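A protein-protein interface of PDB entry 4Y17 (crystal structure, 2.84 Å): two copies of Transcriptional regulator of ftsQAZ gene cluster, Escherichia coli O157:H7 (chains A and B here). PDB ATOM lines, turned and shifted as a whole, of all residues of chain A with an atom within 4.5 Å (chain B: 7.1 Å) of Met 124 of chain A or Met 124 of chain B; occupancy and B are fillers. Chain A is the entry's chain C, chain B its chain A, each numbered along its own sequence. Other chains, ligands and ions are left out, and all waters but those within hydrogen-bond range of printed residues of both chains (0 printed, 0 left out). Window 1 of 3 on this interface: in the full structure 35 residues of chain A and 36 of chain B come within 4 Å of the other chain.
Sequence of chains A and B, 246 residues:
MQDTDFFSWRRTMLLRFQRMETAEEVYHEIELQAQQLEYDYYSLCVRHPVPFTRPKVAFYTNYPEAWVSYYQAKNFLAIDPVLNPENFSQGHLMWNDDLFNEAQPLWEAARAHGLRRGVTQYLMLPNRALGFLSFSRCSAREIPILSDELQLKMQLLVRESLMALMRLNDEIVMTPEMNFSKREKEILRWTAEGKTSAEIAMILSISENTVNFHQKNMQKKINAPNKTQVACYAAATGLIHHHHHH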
ATOM      1  N   LEU A 123      27.334 -10.433   4.789  1.00  0.00           N
ATOM      2  CA  LEU A 123      26.890 -11.065   3.555  1.00  0.00           C
ATOM      3  C   LEU A 123      25.516 -10.538   3.154  1.00  0.00           C
ATOM      4  O   LEU A 123      24.873  -9.811   3.915  1.00  0.00           O
ATOM      5  CB  LEU A 123      26.894 -12.589   3.703  1.00  0.00           C
ATOM      6  CG  LEU A 123      25.805 -13.315   4.494  1.00  0.00           C
ATOM      7  CD1 LEU A 123      24.515 -13.524   3.719  1.00  0.00           C
ATOM      8  CD2 LEU A 123      26.368 -14.648   4.929  1.00  0.00           C
ATOM      9  N   MET A 124      25.073 -10.914   1.959  1.00  0.00           N
ATOM     10  CA  MET A 124      23.770 -10.503   1.448  1.00  0.00           C
ATOM     11  C   MET A 124      22.741 -11.631   1.508  1.00  0.00           C
ATOM     12  O   MET A 124      23.010 -12.753   1.086  1.00  0.00           O
ATOM     13  CB  MET A 124      23.920 -10.014   0.014  1.00  0.00           C
ATOM     14  CG  MET A 124      22.643  -9.491  -0.583  1.00  0.00           C
ATOM     15  SD  MET A 124      22.920  -8.794  -2.210  1.00  0.00           S
ATOM     16  CE  MET A 124      21.243  -8.412  -2.645  1.00  0.00           C
ATOM     17  N   LEU A 125      21.555 -11.313   2.021  1.00  0.00           N
ATOM     18  CA  LEU A 125      20.495 -12.300   2.200  1.00  0.00           C
ATOM     19  C   LEU A 125      19.594 -12.404   0.966  1.00  0.00           C
ATOM     20  O   LEU A 125      19.589 -11.506   0.129  1.00  0.00           O
ATOM     21  CB  LEU A 125      19.656 -11.939   3.427  1.00  0.00           C
ATOM     22  CG  LEU A 125      20.398 -11.914   4.765  1.00  0.00           C
ATOM     23  CD1 LEU A 125      19.514 -11.308   5.844  1.00  0.00           C
ATOM     24  CD2 LEU A 125      20.862 -13.306   5.167  1.00  0.00           C
ATOM     25  N   PRO A 126      18.818 -13.500   0.861  1.00  0.00           N
ATOM     26  CA  PRO A 126      17.897 -13.711  -0.267  1.00  0.00           C
ATOM     27  C   PRO A 126      16.876 -12.591  -0.467  1.00  0.00           C
ATOM     28  O   PRO A 126      16.405 -12.407  -1.589  1.00  0.00           O
ATOM     29  CB  PRO A 126      17.192 -15.019   0.101  1.00  0.00           C
ATOM     30  CG  PRO A 126      18.166 -15.741   0.948  1.00  0.00           C
ATOM     31  CD  PRO A 126      18.878 -14.685   1.738  1.00  0.00           C
ATOM     32  N   ARG A 128      17.686  -9.611  -0.216  1.00  0.00           N
ATOM     33  CA  ARG A 128      18.595  -8.518  -0.558  1.00  0.00           C
ATOM     34  C   ARG A 128      18.981  -7.637   0.628  1.00  0.00           C
ATOM     35  O   ARG A 128      19.597  -6.586   0.445  1.00  0.00           O
ATOM     36  CB  ARG A 128      17.999  -7.625  -1.651  1.00  0.00           C
ATOM     37  CG  ARG A 128      17.089  -8.300  -2.662  1.00  0.00           C
ATOM     38  CD  ARG A 128      17.626  -9.602  -3.201  1.00  0.00           C
ATOM     39  NE  ARG A 128      17.050  -9.870  -4.515  1.00  0.00           N
ATOM     40  CZ  ARG A 128      16.915 -11.076  -5.055  1.00  0.00           C
ATOM     41  NH1 ARG A 128      17.326 -12.156  -4.402  1.00  0.00           N
ATOM     42  NH2 ARG A 128      16.375 -11.196  -6.259  1.00  0.00           N
ATOM     43  N   ALA A 129      18.621  -8.051   1.837  1.00  0.00           N
ATOM     44  CA  ALA A 129      19.058  -7.335   3.027  1.00  0.00           C
ATOM     45  C   ALA A 129      20.531  -7.633   3.301  1.00  0.00           C
ATOM     46  O   ALA A 129      20.987  -8.754   3.088  1.00  0.00           O
ATOM     47  CB  ALA A 129      18.202  -7.719   4.221  1.00  0.00           C
ATOM     48  N   LEU A 130      21.267  -6.628   3.764  1.00  0.00           N
ATOM     49  CA  LEU A 130      22.677  -6.794   4.123  1.00  0.00           C
ATOM     50  C   LEU A 130      22.871  -6.955   5.622  1.00  0.00           C
ATOM     51  O   LEU A 130      22.568  -6.052   6.400  1.00  0.00           O
ATOM     52  CB  LEU A 130      23.521  -5.620   3.623  1.00  0.00           C
ATOM     53  CG  LEU A 130      24.050  -5.718   2.189  1.00  0.00           C
ATOM     54  CD1 LEU A 130      22.968  -6.053   1.176  1.00  0.00           C
ATOM     55  CD2 LEU A 130      24.765  -4.427   1.822  1.00  0.00           C
ATOM     56  N   TYR B 122      26.341 -22.794  -6.188  1.00  0.00           N
ATOM     57  CA  TYR B 122      25.737 -21.532  -6.616  1.00  0.00           C
ATOM     58  C   TYR B 122      25.681 -20.466  -5.519  1.00  0.00           C
ATOM     59  O   TYR B 122      25.694 -20.779  -4.327  1.00  0.00           O
ATOM     60  CB  TYR B 122      24.323 -21.788  -7.150  1.00  0.00           C
ATOM     61  CG  TYR B 122      23.208 -21.377  -6.208  1.00  0.00           C
ATOM     62  CD1 TYR B 122      22.646 -20.107  -6.277  1.00  0.00           C
ATOM     63  CD2 TYR B 122      22.709 -22.261  -5.260  1.00  0.00           C
ATOM     64  CE1 TYR B 122      21.625 -19.728  -5.424  1.00  0.00           C
ATOM     65  CE2 TYR B 122      21.687 -21.889  -4.403  1.00  0.00           C
ATOM     66  CZ  TYR B 122      21.151 -20.623  -4.489  1.00  0.00           C
ATOM     67  OH  TYR B 122      20.136 -20.251  -3.637  1.00  0.00           O
ATOM     68  N   LEU B 123      25.619 -19.204  -5.945  1.00  0.00           N
ATOM     69  CA  LEU B 123      25.429 -18.075  -5.035  1.00  0.00           C
ATOM     70  C   LEU B 123      24.741 -16.904  -5.740  1.00  0.00           C
ATOM     71  O   LEU B 123      24.522 -16.933  -6.954  1.00  0.00           O
ATOM     72  CB  LEU B 123      26.767 -17.600  -4.459  1.00  0.00           C
ATOM     73  CG  LEU B 123      27.635 -16.697  -5.345  1.00  0.00           C
ATOM     74  CD1 LEU B 123      28.898 -16.270  -4.609  1.00  0.00           C
ATOM     75  CD2 LEU B 123      27.980 -17.369  -6.662  1.00  0.00           C
ATOM     76  N   MET B 124      24.394 -15.882  -4.962  1.00  0.00           N
ATOM     77  CA  MET B 124      23.815 -14.659  -5.505  1.00  0.00           C
ATOM     78  C   MET B 124      24.867 -13.559  -5.493  1.00  0.00           C
ATOM     79  O   MET B 124      25.556 -13.362  -4.494  1.00  0.00           O
ATOM     80  CB  MET B 124      22.596 -14.218  -4.699  1.00  0.00           C
ATOM     81  CG  MET B 124      21.898 -12.997  -5.282  1.00  0.00           C
ATOM     82  SD  MET B 124      20.374 -12.549  -4.427  1.00  0.00           S
ATOM     83  CE  MET B 124      20.969 -12.367  -2.748  1.00  0.00           C
ATOM     84  N   LEU B 125      24.993 -12.854  -6.612  1.00  0.00           N
ATOM     85  CA  LEU B 125      25.985 -11.795  -6.752  1.00  0.00           C
ATOM     86  C   LEU B 125      25.398 -10.451  -6.317  1.00  0.00           C
ATOM     87  O   LEU B 125      24.181 -10.325  -6.184  1.00  0.00           O
ATOM     88  CB  LEU B 125      26.481 -11.730  -8.197  1.00  0.00           C
ATOM     89  CG  LEU B 125      27.179 -13.001  -8.691  1.00  0.00           C
ATOM     90  CD1 LEU B 125      27.418 -12.936 -10.189  1.00  0.00           C
ATOM     91  CD2 LEU B 125      28.488 -13.245  -7.945  1.00  0.00           C
ATOM     92  N   PRO B 126      26.261  -9.445  -6.085  1.00  0.00           N
ATOM     93  CA  PRO B 126      25.793  -8.113  -5.675  1.00  0.00           C
ATOM     94  C   PRO B 126      24.777  -7.486  -6.636  1.00  0.00           C
ATOM     95  O   PRO B 126      23.978  -6.662  -6.193  1.00  0.00           O
ATOM     96  CB  PRO B 126      27.083  -7.288  -5.642  1.00  0.00           C
ATOM     97  CG  PRO B 126      28.155  -8.280  -5.367  1.00  0.00           C
ATOM     98  CD  PRO B 126      27.733  -9.530  -6.080  1.00  0.00           C
ATOM     99  N   ASN B 127      24.809  -7.862  -7.914  1.00  0.00           N
ATOM    100  CA  ASN B 127      23.802  -7.405  -8.874  1.00  0.00           C
ATOM    101  C   ASN B 127      22.599  -8.350  -8.925  1.00  0.00           C
ATOM    102  O   ASN B 127      21.798  -8.308  -9.858  1.00  0.00           O
ATOM    103  CB  ASN B 127      24.415  -7.265 -10.271  1.00  0.00           C
ATOM    104  CG  ASN B 127      25.021  -8.560 -10.780  1.00  0.00           C
ATOM    105  OD1 ASN B 127      24.851  -9.622 -10.180  1.00  0.00           O
ATOM    106  ND2 ASN B 127      25.730  -8.476 -11.900  1.00  0.00           N
ATOM    107  N   ARG B 128      22.491  -9.190  -7.899  1.00  0.00           N
ATOM    108  CA  ARG B 128      21.407 -10.162  -7.734  1.00  0.00           C
ATOM    109  C   ARG B 128      21.422 -11.238  -8.816  1.00  0.00           C
ATOM    110  O   ARG B 128      20.475 -12.017  -8.925  1.00  0.00           O
ATOM    111  CB  ARG B 128      20.026  -9.501  -7.745  1.00  0.00           C
ATOM    112  CG  ARG B 128      19.936  -8.059  -7.286  1.00  0.00           C
ATOM    113  CD  ARG B 128      20.751  -7.730  -6.074  1.00  0.00           C
ATOM    114  NE  ARG B 128      20.158  -6.602  -5.361  1.00  0.00           N
ATOM    115  CZ  ARG B 128      20.825  -5.744  -4.598  1.00  0.00           C
ATOM    116  NH1 ARG B 128      20.169  -4.769  -3.992  1.00  0.00           N
ATOM    117  NH2 ARG B 128      22.139  -5.847  -4.444  1.00  0.00           N
ATOM    118  N   ALA B 129      22.485 -11.287  -9.611  1.00  0.00           N
ATOM    119  CA  ALA B 129      22.619 -12.343 -10.603  1.00  0.00           C
ATOM    120  C   ALA B 129      22.930 -13.652  -9.893  1.00  0.00           C
ATOM    121  O   ALA B 129      23.642 -13.673  -8.885  1.00  0.00           O
ATOM    122  CB  ALA B 129      23.704 -12.009 -11.611  1.00  0.00           C
ATOM    123  N   LEU B 130      22.389 -14.743 -10.425  1.00  0.00           N
ATOM    124  CA  LEU B 130      22.599 -16.060  -9.850  1.00  0.00           C
ATOM    125  C   LEU B 130      23.694 -16.780 -10.626  1.00  0.00           C
ATOM    126  O   LEU B 130      23.529 -17.074 -11.808  1.00  0.00           O
ATOM    127  CB  LEU B 130      21.301 -16.866  -9.887  1.00  0.00           C
ATOM    128  CG  LEU B 130      20.244 -16.548  -8.827  1.00  0.00           C
ATOM    129  CD1 LEU B 130      19.032 -17.437  -9.040  1.00  0.00           C
ATOM    130  CD2 LEU B 130      20.775 -16.695  -7.407  1.00  0.00           C
ATOM    131  N   GLY B 131      24.806 -17.067  -9.954  1.00  0.00           N
ATOM    132  CA  GLY B 131      25.939 -17.726 -10.582  1.00  0.00           C
ATOM    133  C   GLY B 131      25.982 -19.208 -10.259  1.00  0.00           C
ATOM    134  O   GLY B 131      25.832 -19.596  -9.104  1.00  0.00           O
ATOM    135  N   MET B 163      33.367 -12.837  -9.071  1.00  0.00           N
ATOM    136  CA  MET B 163      33.702 -11.514  -8.558  1.00  0.00           C
ATOM    137  C   MET B 163      34.872 -10.945  -9.351  1.00  0.00           C
ATOM    138  O   MET B 163      34.910  -9.751  -9.654  1.00  0.00           O
ATOM    139  CB  MET B 163      34.043 -11.575  -7.068  1.00  0.00           C
ATOM    140  CG  MET B 163      32.852 -11.885  -6.160  1.00  0.00           C
ATOM    141  SD  MET B 163      31.538 -10.651  -6.186  1.00  0.00           S
ATOM    142  CE  MET B 163      32.432  -9.163  -5.737  1.00  0.00           C
ATOM    143  N   THR B 237      18.218  -4.942  -9.827  1.00  0.00           N
ATOM    144  CA  THR B 237      19.665  -5.146  -9.918  1.00  0.00           C
ATOM    145  C   THR B 237      20.423  -4.512  -8.754  1.00  0.00           C
ATOM    146  O   THR B 237      21.615  -4.761  -8.578  1.00  0.00           O
ATOM    147  CB  THR B 237      20.239  -4.580 -11.233  1.00  0.00           C
ATOM    148  OG1 THR B 237      19.931  -3.186 -11.335  1.00  0.00           O
ATOM    149  CG2 THR B 237      19.663  -5.317 -12.432  1.00  0.00           C
ATOM    150  N   GLY B 238      19.743  -3.681  -7.971  1.00  0.00           N
ATOM    151  CA  GLY B 238      20.364  -3.068  -6.809  1.00  0.00           C
ATOM    152  C   GLY B 238      21.178  -1.831  -7.146  1.00  0.00           C
ATOM    153  O   GLY B 238      21.943  -1.342  -6.314  1.00  0.00           O
ATOM    154  N   HIS B 241      20.536   0.835  -4.405  1.00  0.00           N
ATOM    155  CA  HIS B 241      21.134   0.591  -3.101  1.00  0.00           C
ATOM    156  C   HIS B 241      22.347  -0.336  -3.156  1.00  0.00           C
ATOM    157  O   HIS B 241      22.384  -1.381  -2.505  1.00  0.00           O
ATOM    158  CB  HIS B 241      20.047   0.043  -2.170  1.00  0.00           C
ATOM    159  CG  HIS B 241      19.185  -1.006  -2.806  1.00  0.00           C
ATOM    160  ND1 HIS B 241      18.308  -0.711  -3.828  1.00  0.00           N
ATOM    161  CD2 HIS B 241      19.050  -2.331  -2.566  1.00  0.00           C
ATOM    162  CE1 HIS B 241      17.677  -1.810  -4.197  1.00  0.00           C
ATOM    163  NE2 HIS B 241      18.107  -2.808  -3.447  1.00  0.00           N
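NH2 of Arg 128 of chain B is in hydrogen-bond range of O of Pro 126 of chain B (2.7 Å).
The guanidinium group of Arg 128 of chain A is in hydrogen-bond range of the backbone carbonyl oxygen of Pro 126 of chain A (3.0 Å).
NH1 of Arg 128 of chain B is in hydrogen-bond range of NE2 of His 241 of chain B, 2.9 Å away.
NH1 of Arg 128 of chain A is in hydrogen-bond range of SD of Met 124 of chain B (3.1 Å).
The side-chain sulfur (SD) of Met 124 of chain A lies close to the guanidinium group (NH2) of Arg 128 of chain B (3.8 Å).
Met 124 of chain A touches its own counterpart, Met 124 of chain B.
Met 124 of chain A touches Arg 128 of chain B, and with the chains exchanged Arg 128 of chain A touches Met 124 of chain B.
Leu 125 of chain A touches Met 124 of chain B, but with the chains exchanged Met 124 of chain A does not touch Leu 125 of chain B (4.4 Å).
Of chain B, only Met 124 (3.97 Å) and Arg 128 (3.3 Å) come within 4 Å of Met 124 of chain A.
Of the printed residues of chain B, Arg 128 of chain A touches Met 124.
Met 124 of chain B touches three residues of chain A.
Of the printed residues of chain A, Arg 128 of chain B touches Met 124 (3.3 Å).
Gly 238 of chain B touches none of the printed residues of chain A.
The nearest residue of chain B that does not touch Met 124 of chain A is Leu 125 of chain B (4.4 Å).
The nearest residue of chain A that does not touch Met 124 of chain B is Pro 126 of chain A (4.2 Å).
Met 124 of chain A touches Met 124 of chain B.
O of Leu 125 of chain A touches CE of Met 124 of chain B, 3.3 Å away.
Of the 7 printed residues of chain A, 3 touch a printed residue of chain B.
Printed residues of chain B that touch a printed residue of chain A: Met 124 and Arg 128.
Hydrophobic or aromatic side chains of chain B within 4 Å of the printed part of chain A: Met 124.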
